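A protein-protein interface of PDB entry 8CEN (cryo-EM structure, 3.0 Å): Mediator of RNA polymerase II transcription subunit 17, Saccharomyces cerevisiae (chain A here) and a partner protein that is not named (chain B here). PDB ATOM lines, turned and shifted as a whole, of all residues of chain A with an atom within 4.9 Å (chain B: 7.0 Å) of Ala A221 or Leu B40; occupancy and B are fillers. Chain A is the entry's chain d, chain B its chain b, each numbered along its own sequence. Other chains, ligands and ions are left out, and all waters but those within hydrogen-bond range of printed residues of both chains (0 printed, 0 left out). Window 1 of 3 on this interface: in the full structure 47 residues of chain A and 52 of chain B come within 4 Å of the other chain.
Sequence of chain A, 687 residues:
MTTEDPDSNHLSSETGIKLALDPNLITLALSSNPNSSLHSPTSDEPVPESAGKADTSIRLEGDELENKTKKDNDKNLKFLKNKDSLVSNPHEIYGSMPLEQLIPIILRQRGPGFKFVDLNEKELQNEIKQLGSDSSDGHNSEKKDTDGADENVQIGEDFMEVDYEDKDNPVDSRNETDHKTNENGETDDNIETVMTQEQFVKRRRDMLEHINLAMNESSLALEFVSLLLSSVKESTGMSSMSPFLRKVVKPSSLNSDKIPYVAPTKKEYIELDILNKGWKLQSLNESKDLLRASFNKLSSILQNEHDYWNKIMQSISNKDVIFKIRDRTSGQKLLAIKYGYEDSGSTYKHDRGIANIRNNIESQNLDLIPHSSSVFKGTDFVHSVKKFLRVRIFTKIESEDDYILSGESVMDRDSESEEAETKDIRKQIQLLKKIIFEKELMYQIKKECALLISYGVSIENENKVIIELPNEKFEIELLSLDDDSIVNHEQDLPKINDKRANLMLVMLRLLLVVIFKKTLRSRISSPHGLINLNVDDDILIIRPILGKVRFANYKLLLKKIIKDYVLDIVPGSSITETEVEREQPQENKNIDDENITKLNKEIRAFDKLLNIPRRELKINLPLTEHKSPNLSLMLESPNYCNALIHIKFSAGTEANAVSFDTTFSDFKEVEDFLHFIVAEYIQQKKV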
ATOM      1  N   GLU A 217       3.432   7.308   6.003  1.00  0.00           N
ATOM      2  CA  GLU A 217       4.279   6.293   6.621  1.00  0.00           C
ATOM      3  C   GLU A 217       4.445   6.539   8.118  1.00  0.00           C
ATOM      4  O   GLU A 217       4.392   5.591   8.918  1.00  0.00           O
ATOM      5  CB  GLU A 217       5.635   6.255   5.921  1.00  0.00           C
ATOM      6  CG  GLU A 217       5.554   5.773   4.483  1.00  0.00           C
ATOM      7  CD  GLU A 217       5.006   4.366   4.366  1.00  0.00           C
ATOM      8  OE1 GLU A 217       5.728   3.411   4.719  1.00  0.00           O
ATOM      9  OE2 GLU A 217       3.848   4.214   3.921  1.00  0.00           O
ATOM     10  N   SER A 218       4.624   7.805   8.515  1.00  0.00           N
ATOM     11  CA  SER A 218       4.744   8.124   9.935  1.00  0.00           C
ATOM     12  C   SER A 218       3.455   7.813  10.686  1.00  0.00           C
ATOM     13  O   SER A 218       3.493   7.300  11.812  1.00  0.00           O
ATOM     14  CB  SER A 218       5.128   9.592  10.109  1.00  0.00           C
ATOM     15  OG  SER A 218       5.073   9.974  11.473  1.00  0.00           O
ATOM     16  N   SER A 219       2.302   8.095  10.072  1.00  0.00           N
ATOM     17  CA  SER A 219       1.028   7.798  10.716  1.00  0.00           C
ATOM     18  C   SER A 219       0.787   6.298  10.806  1.00  0.00           C
ATOM     19  O   SER A 219       0.233   5.820  11.801  1.00  0.00           O
ATOM     20  CB  SER A 219      -0.116   8.480   9.971  1.00  0.00           C
ATOM     21  OG  SER A 219      -0.018   8.261   8.579  1.00  0.00           O
ATOM     22  N   LEU A 220       1.188   5.539   9.781  1.00  0.00           N
ATOM     23  CA  LEU A 220       1.057   4.085   9.845  1.00  0.00           C
ATOM     24  C   LEU A 220       1.908   3.503  10.967  1.00  0.00           C
ATOM     25  O   LEU A 220       1.454   2.617  11.705  1.00  0.00           O
ATOM     26  CB  LEU A 220       1.437   3.463   8.503  1.00  0.00           C
ATOM     27  CG  LEU A 220       0.354   3.479   7.424  1.00  0.00           C
ATOM     28  CD1 LEU A 220       0.908   2.989   6.097  1.00  0.00           C
ATOM     29  CD2 LEU A 220      -0.836   2.638   7.853  1.00  0.00           C
ATOM     30  N   ALA A 221       3.136   4.010  11.126  1.00  0.00           N
ATOM     31  CA  ALA A 221       3.977   3.578  12.240  1.00  0.00           C
ATOM     32  C   ALA A 221       3.358   3.944  13.584  1.00  0.00           C
ATOM     33  O   ALA A 221       3.329   3.118  14.508  1.00  0.00           O
ATOM     34  CB  ALA A 221       5.366   4.196  12.117  1.00  0.00           C
ATOM     35  N   LEU A 222       2.845   5.175  13.700  1.00  0.00           N
ATOM     36  CA  LEU A 222       2.225   5.633  14.940  1.00  0.00           C
ATOM     37  C   LEU A 222       1.020   4.782  15.307  1.00  0.00           C
ATOM     38  O   LEU A 222       0.830   4.431  16.477  1.00  0.00           O
ATOM     39  CB  LEU A 222       1.811   7.098  14.801  1.00  0.00           C
ATOM     40  CG  LEU A 222       0.924   7.667  15.910  1.00  0.00           C
ATOM     41  CD1 LEU A 222       1.652   7.670  17.242  1.00  0.00           C
ATOM     42  CD2 LEU A 222       0.424   9.057  15.550  1.00  0.00           C
ATOM     43  N   GLU A 223       0.208   4.422  14.320  1.00  0.00           N
ATOM     44  CA  GLU A 223      -0.998   3.658  14.598  1.00  0.00           C
ATOM     45  C   GLU A 223      -0.698   2.198  14.884  1.00  0.00           C
ATOM     46  O   GLU A 223      -1.405   1.582  15.687  1.00  0.00           O
ATOM     47  CB  GLU A 223      -1.964   3.812  13.435  1.00  0.00           C
ATOM     48  CG  GLU A 223      -2.457   5.225  13.383  1.00  0.00           C
ATOM     49  CD  GLU A 223      -3.601   5.423  12.451  1.00  0.00           C
ATOM     50  OE1 GLU A 223      -4.157   4.428  11.943  1.00  0.00           O
ATOM     51  OE2 GLU A 223      -3.918   6.599  12.214  1.00  0.00           O
ATOM     52  N   PHE A 224       0.350   1.639  14.271  1.00  0.00           N
ATOM     53  CA  PHE A 224       0.819   0.321  14.684  1.00  0.00           C
ATOM     54  C   PHE A 224       1.265   0.331  16.143  1.00  0.00           C
ATOM     55  O   PHE A 224       0.900  -0.558  16.925  1.00  0.00           O
ATOM     56  CB  PHE A 224       1.959  -0.134  13.775  1.00  0.00           C
ATOM     57  CG  PHE A 224       2.847  -1.164  14.399  1.00  0.00           C
ATOM     58  CD1 PHE A 224       2.388  -2.450  14.631  1.00  0.00           C
ATOM     59  CD2 PHE A 224       4.141  -0.839  14.774  1.00  0.00           C
ATOM     60  CE1 PHE A 224       3.203  -3.389  15.220  1.00  0.00           C
ATOM     61  CE2 PHE A 224       4.958  -1.777  15.359  1.00  0.00           C
ATOM     62  CZ  PHE A 224       4.488  -3.051  15.580  1.00  0.00           C
ATOM     63  N   VAL A 225       2.038   1.352  16.530  1.00  0.00           N
ATOM     64  CA  VAL A 225       2.527   1.436  17.905  1.00  0.00           C
ATOM     65  C   VAL A 225       1.370   1.639  18.880  1.00  0.00           C
ATOM     66  O   VAL A 225       1.345   1.045  19.962  1.00  0.00           O
ATOM     67  CB  VAL A 225       3.586   2.548  18.025  1.00  0.00           C
ATOM     68  CG1 VAL A 225       4.016   2.719  19.453  1.00  0.00           C
ATOM     69  CG2 VAL A 225       4.795   2.202  17.207  1.00  0.00           C
ATOM     70  N   ASP B  34       5.380   3.235  24.646  1.00  0.00           N
ATOM     71  CA  ASP B  34       4.762   4.522  24.953  1.00  0.00           C
ATOM     72  C   ASP B  34       5.651   5.687  24.533  1.00  0.00           C
ATOM     73  O   ASP B  34       5.163   6.668  23.955  1.00  0.00           O
ATOM     74  CB  ASP B  34       4.445   4.605  26.444  1.00  0.00           C
ATOM     75  CG  ASP B  34       3.174   5.378  26.725  1.00  0.00           C
ATOM     76  OD1 ASP B  34       2.709   6.109  25.825  1.00  0.00           O
ATOM     77  OD2 ASP B  34       2.643   5.257  27.848  1.00  0.00           O
ATOM     78  N   ALA B  35       6.956   5.593  24.808  1.00  0.00           N
ATOM     79  CA  ALA B  35       7.876   6.661  24.431  1.00  0.00           C
ATOM     80  C   ALA B  35       7.945   6.823  22.918  1.00  0.00           C
ATOM     81  O   ALA B  35       7.866   7.947  22.396  1.00  0.00           O
ATOM     82  CB  ALA B  35       9.263   6.382  25.011  1.00  0.00           C
ATOM     83  N   VAL B  36       8.063   5.706  22.192  1.00  0.00           N
ATOM     84  CA  VAL B  36       8.148   5.809  20.741  1.00  0.00           C
ATOM     85  C   VAL B  36       6.815   6.276  20.165  1.00  0.00           C
ATOM     86  O   VAL B  36       6.793   6.990  19.161  1.00  0.00           O
ATOM     87  CB  VAL B  36       8.641   4.486  20.109  1.00  0.00           C
ATOM     88  CG1 VAL B  36       7.623   3.375  20.237  1.00  0.00           C
ATOM     89  CG2 VAL B  36       9.024   4.689  18.652  1.00  0.00           C
ATOM     90  N   ARG B  37       5.693   5.967  20.833  1.00  0.00           N
ATOM     91  CA  ARG B  37       4.400   6.475  20.387  1.00  0.00           C
ATOM     92  C   ARG B  37       4.308   7.984  20.548  1.00  0.00           C
ATOM     93  O   ARG B  37       3.777   8.672  19.672  1.00  0.00           O
ATOM     94  CB  ARG B  37       3.270   5.789  21.153  1.00  0.00           C
ATOM     95  CG  ARG B  37       1.882   6.152  20.657  1.00  0.00           C
ATOM     96  CD  ARG B  37       0.833   5.970  21.733  1.00  0.00           C
ATOM     97  NE  ARG B  37       1.089   6.783  22.914  1.00  0.00           N
ATOM     98  CZ  ARG B  37       0.628   8.013  23.091  1.00  0.00           C
ATOM     99  NH1 ARG B  37      -0.091   8.621  22.162  1.00  0.00           N
ATOM    100  NH2 ARG B  37       0.891   8.648  24.228  1.00  0.00           N
ATOM    101  N   MET B  38       4.826   8.517  21.657  1.00  0.00           N
ATOM    102  CA  MET B  38       4.752   9.960  21.881  1.00  0.00           C
ATOM    103  C   MET B  38       5.639  10.729  20.900  1.00  0.00           C
ATOM    104  O   MET B  38       5.186  11.705  20.278  1.00  0.00           O
ATOM    105  CB  MET B  38       5.101  10.276  23.338  1.00  0.00           C
ATOM    106  CG  MET B  38       4.075   9.656  24.290  1.00  0.00           C
ATOM    107  SD  MET B  38       4.612   9.243  25.960  1.00  0.00           S
ATOM    108  CE  MET B  38       5.197  10.822  26.525  1.00  0.00           C
ATOM    109  N   ARG B  39       6.895  10.289  20.717  1.00  0.00           N
ATOM    110  CA  ARG B  39       7.747  10.940  19.715  1.00  0.00           C
ATOM    111  C   ARG B  39       7.199  10.766  18.299  1.00  0.00           C
ATOM    112  O   ARG B  39       7.280  11.688  17.474  1.00  0.00           O
ATOM    113  CB  ARG B  39       9.193  10.437  19.781  1.00  0.00           C
ATOM    114  CG  ARG B  39      10.073  10.983  20.913  1.00  0.00           C
ATOM    115  CD  ARG B  39       9.963  10.260  22.230  1.00  0.00           C
ATOM    116  NE  ARG B  39      10.993  10.694  23.164  1.00  0.00           N
ATOM    117  CZ  ARG B  39      10.828  11.658  24.058  1.00  0.00           C
ATOM    118  NH1 ARG B  39       9.686  12.316  24.158  1.00  0.00           N
ATOM    119  NH2 ARG B  39      11.834  11.971  24.870  1.00  0.00           N
ATOM    120  N   LEU B  40       6.616   9.604  18.003  1.00  0.00           N
ATOM    121  CA  LEU B  40       6.101   9.347  16.667  1.00  0.00           C
ATOM    122  C   LEU B  40       4.841  10.159  16.389  1.00  0.00           C
ATOM    123  O   LEU B  40       4.629  10.604  15.257  1.00  0.00           O
ATOM    124  CB  LEU B  40       5.850   7.848  16.530  1.00  0.00           C
ATOM    125  CG  LEU B  40       5.708   7.188  15.169  1.00  0.00           C
ATOM    126  CD1 LEU B  40       6.755   7.712  14.214  1.00  0.00           C
ATOM    127  CD2 LEU B  40       5.909   5.711  15.398  1.00  0.00           C
ATOM    128  N   ALA B  41       4.014  10.380  17.414  1.00  0.00           N
ATOM    129  CA  ALA B  41       2.862  11.262  17.282  1.00  0.00           C
ATOM    130  C   ALA B  41       3.295  12.704  17.072  1.00  0.00           C
ATOM    131  O   ALA B  41       2.666  13.435  16.298  1.00  0.00           O
ATOM    132  CB  ALA B  41       1.966  11.145  18.514  1.00  0.00           C
ATOM    133  N   GLN B  42       4.362  13.131  17.759  1.00  0.00           N
ATOM    134  CA  GLN B  42       4.905  14.470  17.527  1.00  0.00           C
ATOM    135  C   GLN B  42       5.376  14.633  16.084  1.00  0.00           C
ATOM    136  O   GLN B  42       5.072  15.638  15.423  1.00  0.00           O
ATOM    137  CB  GLN B  42       6.055  14.737  18.498  1.00  0.00           C
ATOM    138  CG  GLN B  42       5.624  15.046  19.919  1.00  0.00           C
ATOM    139  CD  GLN B  42       6.797  15.105  20.878  1.00  0.00           C
ATOM    140  OE1 GLN B  42       7.902  15.489  20.499  1.00  0.00           O
ATOM    141  NE2 GLN B  42       6.563  14.717  22.126  1.00  0.00           N
ATOM    142  N   LEU B  43       6.103  13.631  15.574  1.00  0.00           N
ATOM    143  CA  LEU B  43       6.574  13.664  14.191  1.00  0.00           C
ATOM    144  C   LEU B  43       5.412  13.669  13.200  1.00  0.00           C
ATOM    145  O   LEU B  43       5.431  14.418  12.214  1.00  0.00           O
ATOM    146  CB  LEU B  43       7.497  12.474  13.926  1.00  0.00           C
ATOM    147  CG  LEU B  43       8.002  12.279  12.494  1.00  0.00           C
ATOM    148  CD1 LEU B  43       8.799  13.483  12.029  1.00  0.00           C
ATOM    149  CD2 LEU B  43       8.830  11.010  12.384  1.00  0.00           C
ATOM    150  N   THR B  44       4.389  12.848  13.456  1.00  0.00           N
ATOM    151  CA  THR B  44       3.232  12.786  12.567  1.00  0.00           C
ATOM    152  C   THR B  44       2.460  14.098  12.559  1.00  0.00           C
ATOM    153  O   THR B  44       1.992  14.544  11.506  1.00  0.00           O
ATOM    154  CB  THR B  44       2.314  11.637  12.978  1.00  0.00           C
ATOM    155  OG1 THR B  44       3.094  10.467  13.248  1.00  0.00           O
ATOM    156  CG2 THR B  44       1.320  11.335  11.872  1.00  0.00           C
ATOM    157  N   HIS B  45       2.315  14.734  13.724  1.00  0.00           N
ATOM    158  CA  HIS B  45       1.590  15.998  13.782  1.00  0.00           C
ATOM    159  C   HIS B  45       2.363  17.113  13.085  1.00  0.00           C
ATOM    160  O   HIS B  45       1.763  17.968  12.422  1.00  0.00           O
ATOM    161  CB  HIS B  45       1.290  16.367  15.233  1.00  0.00           C
ATOM    162  CG  HIS B  45       0.508  17.633  15.381  1.00  0.00           C
ATOM    163  ND1 HIS B  45      -0.836  17.717  15.086  1.00  0.00           N
ATOM    164  CD2 HIS B  45       0.880  18.869  15.789  1.00  0.00           C
ATOM    165  CE1 HIS B  45      -1.257  18.949  15.307  1.00  0.00           C
ATOM    166  NE2 HIS B  45      -0.236  19.667  15.736  1.00  0.00           N
ATOM    167  N   SER B  46       3.695  17.119  13.215  1.00  0.00           N
ATOM    168  CA  SER B  46       4.495  18.097  12.480  1.00  0.00           C
ATOM    169  C   SER B  46       4.407  17.875  10.973  1.00  0.00           C
ATOM    170  O   SER B  46       4.329  18.839  10.196  1.00  0.00           O
ATOM    171  CB  SER B  46       5.946  18.045  12.944  1.00  0.00           C
ATOM    172  OG  SER B  46       6.055  18.383  14.315  1.00  0.00           O
ATOM    173  N   GLN B  75      12.503  16.080  15.561  1.00  0.00           N
ATOM    174  CA  GLN B  75      11.649  15.028  16.102  1.00  0.00           C
ATOM    175  C   GLN B  75      11.934  13.678  15.457  1.00  0.00           C
ATOM    176  O   GLN B  75      11.802  12.642  16.118  1.00  0.00           O
ATOM    177  CB  GLN B  75      10.179  15.405  15.945  1.00  0.00           C
ATOM    178  CG  GLN B  75       9.757  16.556  16.837  1.00  0.00           C
ATOM    179  CD  GLN B  75       8.516  17.244  16.331  1.00  0.00           C
ATOM    180  OE1 GLN B  75       8.285  17.337  15.126  1.00  0.00           O
ATOM    181  NE2 GLN B  75       7.699  17.724  17.255  1.00  0.00           N
ATOM    182  N   LEU B  76      12.322  13.665  14.178  1.00  0.00           N
ATOM    183  CA  LEU B  76      12.784  12.422  13.565  1.00  0.00           C
ATOM    184  C   LEU B  76      14.049  11.911  14.248  1.00  0.00           C
ATOM    185  O   LEU B  76      14.181  10.709  14.515  1.00  0.00           O
ATOM    186  CB  LEU B  76      13.023  12.631  12.070  1.00  0.00           C
ATOM    187  CG  LEU B  76      13.461  11.413  11.255  1.00  0.00           C
ATOM    188  CD1 LEU B  76      12.502  10.251  11.457  1.00  0.00           C
ATOM    189  CD2 LEU B  76      13.573  11.768   9.782  1.00  0.00           C
ATOM    190  N   SER B  78      14.830  12.577  17.352  1.00  0.00           N
ATOM    191  CA  SER B  78      14.443  12.177  18.701  1.00  0.00           C
ATOM    192  C   SER B  78      13.787  10.801  18.715  1.00  0.00           C
ATOM    193  O   SER B  78      14.056   9.994  19.610  1.00  0.00           O
ATOM    194  CB  SER B  78      13.509  13.218  19.316  1.00  0.00           C
ATOM    195  OG  SER B  78      12.226  13.162  18.723  1.00  0.00           O
ATOM    196  N   VAL B  79      12.925  10.512  17.736  1.00  0.00           N
ATOM    197  CA  VAL B  79      12.308   9.190  17.700  1.00  0.00           C
ATOM    198  C   VAL B  79      13.332   8.127  17.305  1.00  0.00           C
ATOM    199  O   VAL B  79      13.296   7.004  17.827  1.00  0.00           O
ATOM    200  CB  VAL B  79      11.050   9.184  16.798  1.00  0.00           C
ATOM    201  CG1 VAL B  79      11.382   9.246  15.314  1.00  0.00           C
ATOM    202  CG2 VAL B  79      10.190   7.966  17.099  1.00  0.00           C
ATOM    203  N   LEU B 113      -0.215  -3.020   8.362  1.00  0.00           N
ATOM    204  CA  LEU B 113       0.179  -2.499   9.662  1.00  0.00           C
ATOM    205  C   LEU B 113       1.337  -3.272  10.284  1.00  0.00           C
ATOM    206  O   LEU B 113       2.030  -2.728  11.149  1.00  0.00           O
ATOM    207  CB  LEU B 113      -1.023  -2.499  10.606  1.00  0.00           C
ATOM    208  CG  LEU B 113      -1.062  -1.388  11.655  1.00  0.00           C
ATOM    209  CD1 LEU B 113      -0.705  -0.046  11.032  1.00  0.00           C
ATOM    210  CD2 LEU B 113      -2.437  -1.322  12.276  1.00  0.00           C
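The side-chain hydroxyl of Ser A218 sits at hydrogen-bond distance from the side-chain hydroxyl of Thr B44 (2.7 Å).
The guanidinium group (NE) of Arg B37 lies within salt-bridge range of the side-chain carboxylate (OD1) of Asp B34.
The side-chain hydroxyl (OG1) of Thr B44 sits at hydrogen-bond distance from the backbone carbonyl oxygen (O) of Leu B40.
Among the printed residues, pairs that only touch across the chains: Ser A218 with Leu B40 (3.9 Å), Ser A218 with Leu B43 (3.9 Å), Ser A219 with Thr B44 (3.7 Å), Leu A220 with Leu B113 (3.5 Å), Ala A221 with Leu B40 (3.6 Å), Leu A222 with Arg B37 (3.4 Å), Leu A222 with Leu B40 (3.5 Å), Leu A222 with Ala B41 (3.6 Å), Leu A222 with Thr B44 (3.8 Å), Phe A224 with Leu B113 (3.5 Å), Val A225 with Val B36 (3.7 Å) and Val A225 with Arg B37 (3.6 Å).
Of chain B, only Leu B40 comes within 4 Å of Ala A221.
Of chain A, only Ser A218 (3.9 Å), Ala A221 (3.6 Å) and Leu A222 (3.5 Å) come within 4 Å of Leu B40.
Printed residues of chain A within 4 Å of Arg B37: Leu A222 and Val A225.
Of the printed residues of chain A, Ala B41 touches Leu A222 (3.6 Å).
Printed residues of chain A within 4 Å of Val B36: Val A225.
Printed residues of chain B within 4 Å of Ser A218: Leu B40, Leu B43 and Thr B44.
Of the printed residues of chain A, Leu B43 touches Ser A218 (3.9 Å).
The nearest residue of chain B that does not touch Ala A221 is Leu B113 (5.6 Å).
Printed residues of chain A that touch a printed residue of chain B: Ser A218, Ser A219, Leu A220, Ala A221, Leu A222, Phe A224 and Val A225.
Hydrophobic or aromatic side chains of chain A within 4 Å of the printed part of chain B: Ala A221, Leu A222, Phe A224 and Val A225.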
